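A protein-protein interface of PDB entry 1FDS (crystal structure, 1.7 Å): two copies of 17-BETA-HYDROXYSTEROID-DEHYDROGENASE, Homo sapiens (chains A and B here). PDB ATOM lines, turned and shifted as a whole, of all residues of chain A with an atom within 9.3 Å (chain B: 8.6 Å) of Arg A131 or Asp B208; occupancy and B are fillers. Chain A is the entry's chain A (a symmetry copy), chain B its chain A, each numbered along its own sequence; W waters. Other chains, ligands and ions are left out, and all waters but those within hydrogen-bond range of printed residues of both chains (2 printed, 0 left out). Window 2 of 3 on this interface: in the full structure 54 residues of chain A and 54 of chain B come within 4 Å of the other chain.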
ATOM      1  N   ARG A  76      -3.758  45.692  -8.126  1.00  0.00           N
ATOM      2  CA  ARG A  76      -4.767  44.699  -8.478  1.00  0.00           C
ATOM      3  C   ARG A  76      -6.179  45.257  -8.250  1.00  0.00           C
ATOM      4  O   ARG A  76      -7.112  44.944  -8.998  1.00  0.00           O
ATOM      5  CB  ARG A  76      -4.562  43.434  -7.650  1.00  0.00           C
ATOM      6  CG  ARG A  76      -5.590  42.365  -7.883  1.00  0.00           C
ATOM      7  CD  ARG A  76      -5.408  41.242  -6.904  1.00  0.00           C
ATOM      8  NE  ARG A  76      -6.645  40.498  -6.757  1.00  0.00           N
ATOM      9  CZ  ARG A  76      -6.927  39.729  -5.715  1.00  0.00           C
ATOM     10  NH1 ARG A  76      -6.041  39.598  -4.725  1.00  0.00           N
ATOM     11  NH2 ARG A  76      -8.107  39.117  -5.646  1.00  0.00           N
ATOM     12  N   GLN A 123       1.383  35.296  -6.905  1.00  0.00           N
ATOM     13  CA  GLN A 123       0.577  34.997  -5.735  1.00  0.00           C
ATOM     14  C   GLN A 123      -0.669  35.866  -5.741  1.00  0.00           C
ATOM     15  O   GLN A 123      -1.733  35.408  -5.341  1.00  0.00           O
ATOM     16  CB  GLN A 123       1.346  35.211  -4.431  1.00  0.00           C
ATOM     17  CG  GLN A 123       2.467  34.236  -4.230  1.00  0.00           C
ATOM     18  CD  GLN A 123       3.189  34.442  -2.922  1.00  0.00           C
ATOM     19  OE1 GLN A 123       3.442  33.494  -2.170  1.00  0.00           O
ATOM     20  NE2 GLN A 123       3.549  35.664  -2.651  1.00  0.00           N
ATOM     21  N   ALA A 124      -0.553  37.096  -6.223  1.00  0.00           N
ATOM     22  CA  ALA A 124      -1.687  38.003  -6.250  1.00  0.00           C
ATOM     23  C   ALA A 124      -2.682  37.725  -7.360  1.00  0.00           C
ATOM     24  O   ALA A 124      -3.887  37.859  -7.148  1.00  0.00           O
ATOM     25  CB  ALA A 124      -1.214  39.451  -6.348  1.00  0.00           C
ATOM     26  N   PHE A 125      -2.196  37.295  -8.524  1.00  0.00           N
ATOM     27  CA  PHE A 125      -3.063  37.091  -9.677  1.00  0.00           C
ATOM     28  C   PHE A 125      -3.410  35.684 -10.065  1.00  0.00           C
ATOM     29  O   PHE A 125      -4.437  35.452 -10.677  1.00  0.00           O
ATOM     30  CB  PHE A 125      -2.469  37.836 -10.891  1.00  0.00           C
ATOM     31  CG  PHE A 125      -2.486  39.331 -10.734  1.00  0.00           C
ATOM     32  CD1 PHE A 125      -3.590  40.069 -11.132  1.00  0.00           C
ATOM     33  CD2 PHE A 125      -1.434  39.987 -10.128  1.00  0.00           C
ATOM     34  CE1 PHE A 125      -3.643  41.451 -10.918  1.00  0.00           C
ATOM     35  CE2 PHE A 125      -1.471  41.349  -9.911  1.00  0.00           C
ATOM     36  CZ  PHE A 125      -2.582  42.091 -10.307  1.00  0.00           C
ATOM     37  N   LEU A 126      -2.541  34.737  -9.760  1.00  0.00           N
ATOM     38  CA  LEU A 126      -2.799  33.364 -10.137  1.00  0.00           C
ATOM     39  C   LEU A 126      -4.073  32.723  -9.547  1.00  0.00           C
ATOM     40  O   LEU A 126      -4.777  32.009 -10.246  1.00  0.00           O
ATOM     41  CB  LEU A 126      -1.560  32.506  -9.829  1.00  0.00           C
ATOM     42  CG  LEU A 126      -1.052  31.494 -10.854  1.00  0.00           C
ATOM     43  CD1 LEU A 126      -2.050  30.388 -10.974  1.00  0.00           C
ATOM     44  CD2 LEU A 126      -0.822  32.115 -12.229  1.00  0.00           C
ATOM     45  N   PRO A 127      -4.392  32.974  -8.267  1.00  0.00           N
ATOM     46  CA  PRO A 127      -5.601  32.352  -7.711  1.00  0.00           C
ATOM     47  C   PRO A 127      -6.863  32.595  -8.533  1.00  0.00           C
ATOM     48  O   PRO A 127      -7.613  31.664  -8.828  1.00  0.00           O
ATOM     49  CB  PRO A 127      -5.683  32.962  -6.319  1.00  0.00           C
ATOM     50  CG  PRO A 127      -4.240  33.095  -5.939  1.00  0.00           C
ATOM     51  CD  PRO A 127      -3.663  33.707  -7.216  1.00  0.00           C
ATOM     52  N   ASP A 128      -7.067  33.839  -8.924  1.00  0.00           N
ATOM     53  CA  ASP A 128      -8.208  34.230  -9.741  1.00  0.00           C
ATOM     54  C   ASP A 128      -8.250  33.478 -11.063  1.00  0.00           C
ATOM     55  O   ASP A 128      -9.301  33.061 -11.521  1.00  0.00           O
ATOM     56  CB  ASP A 128      -8.078  35.698 -10.069  1.00  0.00           C
ATOM     57  CG  ASP A 128      -9.277  36.453  -9.705  1.00  0.00           C
ATOM     58  OD1 ASP A 128     -10.232  36.482 -10.531  1.00  0.00           O
ATOM     59  OD2 ASP A 128      -9.259  37.003  -8.578  1.00  0.00           O
ATOM     60  N   MET A 129      -7.099  33.342 -11.703  1.00  0.00           N
ATOM     61  CA  MET A 129      -7.048  32.665 -12.970  1.00  0.00           C
ATOM     62  C   MET A 129      -7.362  31.199 -12.796  1.00  0.00           C
ATOM     63  O   MET A 129      -7.998  30.601 -13.654  1.00  0.00           O
ATOM     64  CB  MET A 129      -5.677  32.841 -13.612  1.00  0.00           C
ATOM     65  CG  MET A 129      -5.280  34.286 -13.855  1.00  0.00           C
ATOM     66  SD  MET A 129      -3.709  34.301 -14.730  1.00  0.00           S
ATOM     67  CE  MET A 129      -3.589  36.042 -15.020  1.00  0.00           C
ATOM     68  N   LYS A 130      -6.843  30.600 -11.731  1.00  0.00           N
ATOM     69  CA  LYS A 130      -7.121  29.185 -11.443  1.00  0.00           C
ATOM     70  C   LYS A 130      -8.631  28.969 -11.267  1.00  0.00           C
ATOM     71  O   LYS A 130      -9.185  27.998 -11.779  1.00  0.00           O
ATOM     72  CB  LYS A 130      -6.428  28.746 -10.159  1.00  0.00           C
ATOM     73  CG  LYS A 130      -4.966  28.520 -10.312  1.00  0.00           C
ATOM     74  CD  LYS A 130      -4.362  28.309  -8.947  1.00  0.00           C
ATOM     75  CE  LYS A 130      -3.518  27.097  -8.939  1.00  0.00           C
ATOM     76  NZ  LYS A 130      -3.007  26.906  -7.575  1.00  0.00           N
ATOM     77  N   ARG A 131      -9.265  29.876 -10.522  1.00  0.00           N
ATOM     78  CA  ARG A 131     -10.709  29.836 -10.253  1.00  0.00           C
ATOM     79  C   ARG A 131     -11.502  29.886 -11.553  1.00  0.00           C
ATOM     80  O   ARG A 131     -12.386  29.066 -11.774  1.00  0.00           O
ATOM     81  CB  ARG A 131     -11.116  31.023  -9.373  1.00  0.00           C
ATOM     82  CG  ARG A 131     -11.520  30.659  -7.945  1.00  0.00           C
ATOM     83  CD  ARG A 131     -10.541  29.649  -7.317  1.00  0.00           C
ATOM     84  NE  ARG A 131     -10.758  29.427  -5.880  1.00  0.00           N
ATOM     85  CZ  ARG A 131     -10.122  30.082  -4.901  1.00  0.00           C
ATOM     86  NH1 ARG A 131      -9.220  31.026  -5.179  1.00  0.00           N
ATOM     87  NH2 ARG A 131     -10.343  29.750  -3.632  1.00  0.00           N
ATOM     88  N   ARG A 132     -11.174  30.846 -12.416  1.00  0.00           N
ATOM     89  CA  ARG A 132     -11.867  31.017 -13.687  1.00  0.00           C
ATOM     90  C   ARG A 132     -11.558  29.913 -14.676  1.00  0.00           C
ATOM     91  O   ARG A 132     -12.298  29.710 -15.630  1.00  0.00           O
ATOM     92  CB  ARG A 132     -11.534  32.394 -14.283  1.00  0.00           C
ATOM     93  CG  ARG A 132     -11.866  33.559 -13.349  1.00  0.00           C
ATOM     94  CD  ARG A 132     -11.753  34.923 -14.035  1.00  0.00           C
ATOM     95  NE  ARG A 132     -12.170  36.027 -13.161  1.00  0.00           N
ATOM     96  CZ  ARG A 132     -13.258  36.773 -13.353  1.00  0.00           C
ATOM     97  NH1 ARG A 132     -14.057  36.546 -14.389  1.00  0.00           N
ATOM     98  NH2 ARG A 132     -13.551  37.759 -12.515  1.00  0.00           N
ATOM     99  N   GLY A 133     -10.422  29.254 -14.506  1.00  0.00           N
ATOM    100  CA  GLY A 133     -10.029  28.231 -15.452  1.00  0.00           C
ATOM    101  C   GLY A 133      -9.441  28.851 -16.720  1.00  0.00           C
ATOM    102  O   GLY A 133      -9.454  28.240 -17.794  1.00  0.00           O
ATOM    103  N   SER A 134      -8.945  30.081 -16.627  1.00  0.00           N
ATOM    104  CA  SER A 134      -8.333  30.706 -17.799  1.00  0.00           C
ATOM    105  C   SER A 134      -7.429  31.859 -17.409  1.00  0.00           C
ATOM    106  O   SER A 134      -7.616  32.498 -16.380  1.00  0.00           O
ATOM    107  CB  SER A 134      -9.368  31.168 -18.827  1.00  0.00           C
ATOM    108  OG  SER A 134     -10.028  32.342 -18.396  1.00  0.00           O
ATOM    109  N   GLY A 135      -6.462  32.125 -18.267  1.00  0.00           N
ATOM    110  CA  GLY A 135      -5.532  33.202 -18.003  1.00  0.00           C
ATOM    111  C   GLY A 135      -4.227  32.861 -18.678  1.00  0.00           C
ATOM    112  O   GLY A 135      -3.934  31.683 -18.929  1.00  0.00           O
ATOM    113  N   LEU A 172       2.187  21.995 -12.814  1.00  0.00           N
ATOM    114  CA  LEU A 172       0.960  21.993 -12.043  1.00  0.00           C
ATOM    115  C   LEU A 172      -0.231  22.602 -12.805  1.00  0.00           C
ATOM    116  O   LEU A 172      -1.343  22.055 -12.766  1.00  0.00           O
ATOM    117  CB  LEU A 172       1.172  22.765 -10.731  1.00  0.00           C
ATOM    118  CG  LEU A 172      -0.091  23.024  -9.894  1.00  0.00           C
ATOM    119  CD1 LEU A 172      -0.744  21.705  -9.455  1.00  0.00           C
ATOM    120  CD2 LEU A 172       0.266  23.872  -8.706  1.00  0.00           C
ATOM    121  N   LEU A 173       0.010  23.725 -13.492  1.00  0.00           N
ATOM    122  CA  LEU A 173      -1.030  24.474 -14.203  1.00  0.00           C
ATOM    123  C   LEU A 173      -1.676  23.830 -15.414  1.00  0.00           C
ATOM    124  O   LEU A 173      -2.746  24.245 -15.818  1.00  0.00           O
ATOM    125  CB  LEU A 173      -0.502  25.849 -14.604  1.00  0.00           C
ATOM    126  CG  LEU A 173      -0.165  26.774 -13.440  1.00  0.00           C
ATOM    127  CD1 LEU A 173       0.368  28.080 -14.005  1.00  0.00           C
ATOM    128  CD2 LEU A 173      -1.391  27.012 -12.587  1.00  0.00           C
ATOM    129  N   PHE A 176      -5.355  23.297 -15.177  1.00  0.00           N
ATOM    130  CA  PHE A 176      -6.164  24.444 -14.797  1.00  0.00           C
ATOM    131  C   PHE A 176      -6.557  25.359 -15.951  1.00  0.00           C
ATOM    132  O   PHE A 176      -7.360  26.271 -15.778  1.00  0.00           O
ATOM    133  CB  PHE A 176      -5.452  25.261 -13.746  1.00  0.00           C
ATOM    134  CG  PHE A 176      -5.328  24.567 -12.440  1.00  0.00           C
ATOM    135  CD1 PHE A 176      -4.351  23.599 -12.241  1.00  0.00           C
ATOM    136  CD2 PHE A 176      -6.179  24.890 -11.400  1.00  0.00           C
ATOM    137  CE1 PHE A 176      -4.220  22.959 -11.014  1.00  0.00           C
ATOM    138  CE2 PHE A 176      -6.058  24.258 -10.167  1.00  0.00           C
ATOM    139  CZ  PHE A 176      -5.074  23.293  -9.977  1.00  0.00           C
ATOM    140  N   GLY A 177      -5.978  25.140 -17.120  1.00  0.00           N
ATOM    141  CA  GLY A 177      -6.315  26.005 -18.235  1.00  0.00           C
ATOM    142  C   GLY A 177      -5.618  27.356 -18.148  1.00  0.00           C
ATOM    143  O   GLY A 177      -5.999  28.279 -18.873  1.00  0.00           O
ATOM    144  N   VAL A 178      -4.631  27.486 -17.256  1.00  0.00           N
ATOM    145  CA  VAL A 178      -3.861  28.731 -17.098  1.00  0.00           C
ATOM    146  C   VAL A 178      -2.536  28.453 -17.793  1.00  0.00           C
ATOM    147  O   VAL A 178      -1.869  27.466 -17.500  1.00  0.00           O
ATOM    148  CB  VAL A 178      -3.619  29.093 -15.607  1.00  0.00           C
ATOM    149  CG1 VAL A 178      -2.803  30.408 -15.491  1.00  0.00           C
ATOM    150  CG2 VAL A 178      -4.973  29.226 -14.862  1.00  0.00           C
ATOM    151  N   PRO B  98       1.754  24.906  -2.454  1.00  0.00           N
ATOM    152  CA  PRO B  98       1.199  25.680  -3.571  1.00  0.00           C
ATOM    153  C   PRO B  98       1.816  27.062  -3.438  1.00  0.00           C
ATOM    154  O   PRO B  98       1.864  27.608  -2.337  1.00  0.00           O
ATOM    155  CB  PRO B  98      -0.297  25.742  -3.239  1.00  0.00           C
ATOM    156  CG  PRO B  98      -0.539  24.480  -2.396  1.00  0.00           C
ATOM    157  CD  PRO B  98       0.704  24.427  -1.528  1.00  0.00           C
ATOM    158  N   GLU B 100       0.758  30.101  -3.962  1.00  0.00           N
ATOM    159  CA  GLU B 100      -0.099  31.086  -3.289  1.00  0.00           C
ATOM    160  C   GLU B 100      -0.279  30.860  -1.771  1.00  0.00           C
ATOM    161  O   GLU B 100      -0.774  31.746  -1.061  1.00  0.00           O
ATOM    162  CB  GLU B 100      -1.468  31.203  -3.993  1.00  0.00           C
ATOM    163  CG  GLU B 100      -2.338  29.975  -3.875  1.00  0.00           C
ATOM    164  CD  GLU B 100      -2.127  28.976  -5.009  1.00  0.00           C
ATOM    165  OE1 GLU B 100      -1.028  28.890  -5.582  1.00  0.00           O
ATOM    166  OE2 GLU B 100      -3.076  28.256  -5.345  1.00  0.00           O
ATOM    167  N   ALA B 101       0.133  29.693  -1.278  1.00  0.00           N
ATOM    168  CA  ALA B 101       0.025  29.377   0.138  1.00  0.00           C
ATOM    169  C   ALA B 101       1.299  29.711   0.911  1.00  0.00           C
ATOM    170  O   ALA B 101       1.330  29.589   2.148  1.00  0.00           O
ATOM    171  CB  ALA B 101      -0.308  27.909   0.322  1.00  0.00           C
ATOM    172  N   PHE B 151       5.026  22.189  -7.006  1.00  0.00           N
ATOM    173  CA  PHE B 151       4.971  22.471  -5.582  1.00  0.00           C
ATOM    174  C   PHE B 151       6.318  22.764  -4.947  1.00  0.00           C
ATOM    175  O   PHE B 151       6.394  22.944  -3.747  1.00  0.00           O
ATOM    176  CB  PHE B 151       4.230  21.345  -4.832  1.00  0.00           C
ATOM    177  CG  PHE B 151       2.805  21.206  -5.259  1.00  0.00           C
ATOM    178  CD1 PHE B 151       1.902  22.224  -5.004  1.00  0.00           C
ATOM    179  CD2 PHE B 151       2.387  20.085  -5.951  1.00  0.00           C
ATOM    180  CE1 PHE B 151       0.579  22.140  -5.429  1.00  0.00           C
ATOM    181  CE2 PHE B 151       1.056  19.979  -6.395  1.00  0.00           C
ATOM    182  CZ  PHE B 151       0.158  21.010  -6.129  1.00  0.00           C
ATOM    183  N   VAL B 203      -2.779  24.769   4.585  1.00  0.00           N
ATOM    184  CA  VAL B 203      -2.659  24.759   3.138  1.00  0.00           C
ATOM    185  C   VAL B 203      -4.010  24.920   2.460  1.00  0.00           C
ATOM    186  O   VAL B 203      -4.142  25.723   1.536  1.00  0.00           O
ATOM    187  CB  VAL B 203      -1.985  23.473   2.622  1.00  0.00           C
ATOM    188  CG1 VAL B 203      -1.941  23.469   1.102  1.00  0.00           C
ATOM    189  CG2 VAL B 203      -0.586  23.361   3.187  1.00  0.00           C
ATOM    190  N   LEU B 204      -5.013  24.170   2.917  1.00  0.00           N
ATOM    191  CA  LEU B 204      -6.342  24.248   2.317  1.00  0.00           C
ATOM    192  C   LEU B 204      -6.905  25.637   2.477  1.00  0.00           C
ATOM    193  O   LEU B 204      -7.599  26.126   1.595  1.00  0.00           O
ATOM    194  CB  LEU B 204      -7.315  23.262   2.959  1.00  0.00           C
ATOM    195  CG  LEU B 204      -8.291  22.568   2.006  1.00  0.00           C
ATOM    196  CD1 LEU B 204      -9.482  22.118   2.811  1.00  0.00           C
ATOM    197  CD2 LEU B 204      -8.730  23.427   0.834  1.00  0.00           C
ATOM    198  N   ASP B 205      -6.618  26.259   3.610  1.00  0.00           N
ATOM    199  CA  ASP B 205      -7.106  27.606   3.871  1.00  0.00           C
ATOM    200  C   ASP B 205      -6.538  28.639   2.893  1.00  0.00           C
ATOM    201  O   ASP B 205      -7.179  29.648   2.598  1.00  0.00           O
ATOM    202  CB  ASP B 205      -6.762  28.019   5.308  1.00  0.00           C
ATOM    203  CG  ASP B 205      -7.975  28.485   6.088  1.00  0.00           C
ATOM    204  OD1 ASP B 205      -9.069  27.899   5.909  1.00  0.00           O
ATOM    205  OD2 ASP B 205      -7.834  29.435   6.891  1.00  0.00           O
ATOM    206  N   ARG B 206      -5.358  28.364   2.348  1.00  0.00           N
ATOM    207  CA  ARG B 206      -4.716  29.303   1.442  1.00  0.00           C
ATOM    208  C   ARG B 206      -4.732  28.949  -0.040  1.00  0.00           C
ATOM    209  O   ARG B 206      -4.132  29.662  -0.851  1.00  0.00           O
ATOM    210  CB  ARG B 206      -3.289  29.550   1.911  1.00  0.00           C
ATOM    211  CG  ARG B 206      -3.220  30.134   3.306  1.00  0.00           C
ATOM    212  CD  ARG B 206      -1.797  30.139   3.842  1.00  0.00           C
ATOM    213  NE  ARG B 206      -1.720  30.770   5.158  1.00  0.00           N
ATOM    214  CZ  ARG B 206      -2.053  30.180   6.309  1.00  0.00           C
ATOM    215  NH1 ARG B 206      -2.490  28.918   6.337  1.00  0.00           N
ATOM    216  NH2 ARG B 206      -1.997  30.876   7.442  1.00  0.00           N
ATOM    217  N   THR B 207      -5.394  27.861  -0.416  1.00  0.00           N
ATOM    218  CA  THR B 207      -5.438  27.511  -1.824  1.00  0.00           C
ATOM    219  C   THR B 207      -6.823  26.979  -2.168  1.00  0.00           C
ATOM    220  O   THR B 207      -7.727  27.068  -1.359  1.00  0.00           O
ATOM    221  CB  THR B 207      -4.314  26.505  -2.187  1.00  0.00           C
ATOM    222  OG1 THR B 207      -4.213  26.404  -3.607  1.00  0.00           O
ATOM    223  CG2 THR B 207      -4.586  25.131  -1.620  1.00  0.00           C
ATOM    224  N   ASP B 208      -7.032  26.518  -3.390  1.00  0.00           N
ATOM    225  CA  ASP B 208      -8.328  25.962  -3.743  1.00  0.00           C
ATOM    226  C   ASP B 208      -8.307  24.442  -3.548  1.00  0.00           C
ATOM    227  O   ASP B 208      -7.249  23.808  -3.466  1.00  0.00           O
ATOM    228  CB  ASP B 208      -8.695  26.307  -5.163  1.00  0.00           C
ATOM    229  CG  ASP B 208      -7.711  25.796  -6.139  1.00  0.00           C
ATOM    230  OD1 ASP B 208      -6.651  26.424  -6.292  1.00  0.00           O
ATOM    231  OD2 ASP B 208      -7.988  24.750  -6.744  1.00  0.00           O
ATOM    232  N   ILE B 209      -9.489  23.853  -3.494  1.00  0.00           N
ATOM    233  CA  ILE B 209      -9.631  22.420  -3.304  1.00  0.00           C
ATOM    234  C   ILE B 209      -8.952  21.571  -4.403  1.00  0.00           C
ATOM    235  O   ILE B 209      -8.447  20.486  -4.115  1.00  0.00           O
ATOM    236  CB  ILE B 209     -11.161  22.084  -3.133  1.00  0.00           C
ATOM    237  CG1 ILE B 209     -11.379  21.011  -2.058  1.00  0.00           C
ATOM    238  CG2 ILE B 209     -11.835  21.858  -4.475  1.00  0.00           C
ATOM    239  CD1 ILE B 209     -10.675  19.732  -2.279  1.00  0.00           C
ATOM    240  N   HIS B 210      -8.915  22.052  -5.643  1.00  0.00           N
ATOM    241  CA  HIS B 210      -8.284  21.299  -6.733  1.00  0.00           C
ATOM    242  C   HIS B 210      -6.754  21.276  -6.606  1.00  0.00           C
ATOM    243  O   HIS B 210      -6.122  20.237  -6.820  1.00  0.00           O
ATOM    244  CB  HIS B 210      -8.703  21.862  -8.071  1.00  0.00           C
ATOM    245  CG  HIS B 210     -10.184  21.995  -8.184  1.00  0.00           C
ATOM    246  ND1 HIS B 210     -11.023  20.902  -8.151  1.00  0.00           N
ATOM    247  CD2 HIS B 210     -10.986  23.087  -8.175  1.00  0.00           C
ATOM    248  CE1 HIS B 210     -12.278  21.316  -8.110  1.00  0.00           C
ATOM    249  NE2 HIS B 210     -12.284  22.637  -8.122  1.00  0.00           N
ATOM    250  N   THR B 211      -6.182  22.427  -6.239  1.00  0.00           N
ATOM    251  CA  THR B 211      -4.736  22.542  -6.027  1.00  0.00           C
ATOM    252  C   THR B 211      -4.383  21.676  -4.821  1.00  0.00           C
ATOM    253  O   THR B 211      -3.419  20.922  -4.853  1.00  0.00           O
ATOM    254  CB  THR B 211      -4.314  24.010  -5.770  1.00  0.00           C
ATOM    255  OG1 THR B 211      -4.617  24.787  -6.931  1.00  0.00           O
ATOM    256  CG2 THR B 211      -2.804  24.098  -5.505  1.00  0.00           C
ATOM    257  N   PHE B 212      -5.211  21.736  -3.787  1.00  0.00           N
ATOM    258  CA  PHE B 212      -4.979  20.936  -2.597  1.00  0.00           C
ATOM    259  C   PHE B 212      -4.968  19.448  -2.960  1.00  0.00           C
ATOM    260  O   PHE B 212      -4.135  18.670  -2.481  1.00  0.00           O
ATOM    261  CB  PHE B 212      -6.062  21.206  -1.573  1.00  0.00           C
ATOM    262  CG  PHE B 212      -5.824  20.518  -0.275  1.00  0.00           C
ATOM    263  CD1 PHE B 212      -4.895  21.026   0.633  1.00  0.00           C
ATOM    264  CD2 PHE B 212      -6.503  19.349   0.042  1.00  0.00           C
ATOM    265  CE1 PHE B 212      -4.652  20.373   1.845  1.00  0.00           C
ATOM    266  CE2 PHE B 212      -6.262  18.690   1.251  1.00  0.00           C
ATOM    267  CZ  PHE B 212      -5.337  19.207   2.150  1.00  0.00           C
ATOM    268  N   HIS B 213      -5.892  19.050  -3.814  1.00  0.00           N
ATOM    269  CA  HIS B 213      -5.959  17.674  -4.230  1.00  0.00           C
ATOM    270  C   HIS B 213      -4.681  17.270  -4.963  1.00  0.00           C
ATOM    271  O   HIS B 213      -4.141  16.176  -4.751  1.00  0.00           O
ATOM    272  CB  HIS B 213      -7.172  17.465  -5.136  1.00  0.00           C
ATOM    273  CG  HIS B 213      -7.376  16.039  -5.524  1.00  0.00           C
ATOM    274  ND1 HIS B 213      -7.121  15.568  -6.799  1.00  0.00           N
ATOM    275  CD2 HIS B 213      -7.756  14.963  -4.793  1.00  0.00           C
ATOM    276  CE1 HIS B 213      -7.331  14.264  -6.833  1.00  0.00           C
ATOM    277  NE2 HIS B 213      -7.719  13.872  -5.631  1.00  0.00           N
ATOM    278  N   ARG B 214      -4.221  18.123  -5.873  1.00  0.00           N
ATOM    279  CA  ARG B 214      -3.004  17.838  -6.622  1.00  0.00           C
ATOM    280  C   ARG B 214      -1.808  17.783  -5.666  1.00  0.00           C
ATOM    281  O   ARG B 214      -0.880  17.009  -5.888  1.00  0.00           O
ATOM    282  CB  ARG B 214      -2.755  18.919  -7.671  1.00  0.00           C
ATOM    283  CG  ARG B 214      -3.759  18.959  -8.784  1.00  0.00           C
ATOM    284  CD  ARG B 214      -3.734  17.696  -9.542  1.00  0.00           C
ATOM    285  NE  ARG B 214      -4.614  17.805 -10.691  1.00  0.00           N
ATOM    286  CZ  ARG B 214      -4.984  16.783 -11.459  1.00  0.00           C
ATOM    287  NH1 ARG B 214      -4.556  15.543 -11.207  1.00  0.00           N
ATOM    288  NH2 ARG B 214      -5.766  17.014 -12.514  1.00  0.00           N
ATOM    289  N   PHE B 215      -1.847  18.575  -4.600  1.00  0.00           N
ATOM    290  CA  PHE B 215      -0.755  18.594  -3.622  1.00  0.00           C
ATOM    291  C   PHE B 215      -0.665  17.225  -2.968  1.00  0.00           C
ATOM    292  O   PHE B 215       0.428  16.678  -2.785  1.00  0.00           O
ATOM    293  CB  PHE B 215      -0.969  19.675  -2.564  1.00  0.00           C
ATOM    294  CG  PHE B 215       0.229  19.902  -1.661  1.00  0.00           C
ATOM    295  CD1 PHE B 215       1.538  19.787  -2.151  1.00  0.00           C
ATOM    296  CD2 PHE B 215       0.047  20.257  -0.331  1.00  0.00           C
ATOM    297  CE1 PHE B 215       2.651  20.029  -1.321  1.00  0.00           C
ATOM    298  CE2 PHE B 215       1.148  20.503   0.510  1.00  0.00           C
ATOM    299  CZ  PHE B 215       2.451  20.386   0.007  1.00  0.00           C
HETATM  300  O   HOH W   1      -7.692  29.519  -7.190  1.00  0.00           O
HETATM  301  O   HOH W   2      -0.270  26.876  -7.458  1.00  0.00           O
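The side-chain carboxylate (OE2) of Glu B100 is in salt-bridge range of the side-chain amino group (NZ) of Lys A130 (2.6 Å). The side-chain carboxylate (OD1) of Asp B208 is in salt-bridge range of the side-chain amino group (NZ) of Lys A130 (3.9 Å). OG1 of Thr B211 is in hydrogen-bond range of NZ of Lys A130 (2.7 Å).
OG1 of Thr B207 is in hydrogen-bond range of OE2 of Glu B100, 2.8 Å away. N of His B210 is in hydrogen-bond range of OD2 of Asp B208 (3.1 Å). OG1 of Thr B211 sits at hydrogen-bond distance from OD1 of Asp B208, at 2.7 Å.
CB of Glu B100 touches CG of Pro A127 (3.9 Å). Arg A131 touches Asp B208. CD1 of Leu A172 touches CZ of Phe B151, 3.5 Å away. CD1 of Leu A172 touches CB of Arg B214, 3.9 Å away. Asp B208 touches Phe A176. CZ of Phe A176 touches OG1 of Thr B211, 3.4 Å away.
Of the printed residues of chain B, Pro A127 touches Glu B100. Met A129 touches none of the printed residues of chain B. Arg A131 touches just one residue of chain B: Asp B208 (3.8 Å). Of the printed residues of chain B, Phe A176 touches Asp B208 and Thr B211. No residue of chain A comes within 4 Å of Thr B207. Of chain A, only Lys A130 and Phe A176 come within 4 Å of Thr B211. Printed residues of chain A within 4 Å of Arg B214: Leu A172. Phe B215 touches none of the printed residues of chain A. The nearest residue of chain B that does not touch Arg A131 is Thr B207 (4.4 Å). The nearest residue of chain A that does not touch Asp B208 is Pro A127 (5.9 Å).
Printed residues of chain B that touch a printed residue of chain A: Glu B100, Phe B151, Asp B208, Thr B211 and Arg B214. Of the 19 printed residues of chain A, 5 touch a printed residue of chain B. Printed residues of chain A that touch a printed residue of chain B: Pro A127, Lys A130, Arg A131, Leu A172 and Phe A176. Among the printed residues, Asp or Glu carboxylates within 4 Å of a Lys or Arg side-chain nitrogen of the other chain: Lys A130 with Glu B100 (2.6 Å) and Lys A130 with Asp B208 (3.9 Å).
No position is printed for both chains. Of the 9 pairs that touch across the chains among the printed residues, none has its exchanged pair printed and touching as well.
Water W1 lies within hydrogen-bond range of O of Pro A127, NH1 of Arg A131 and OD1 of Asp B208. Water W2 lies within hydrogen-bond range of NZ of Lys A130 (2.7 Å) and OE1 of Glu B100 (2.9 Å).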
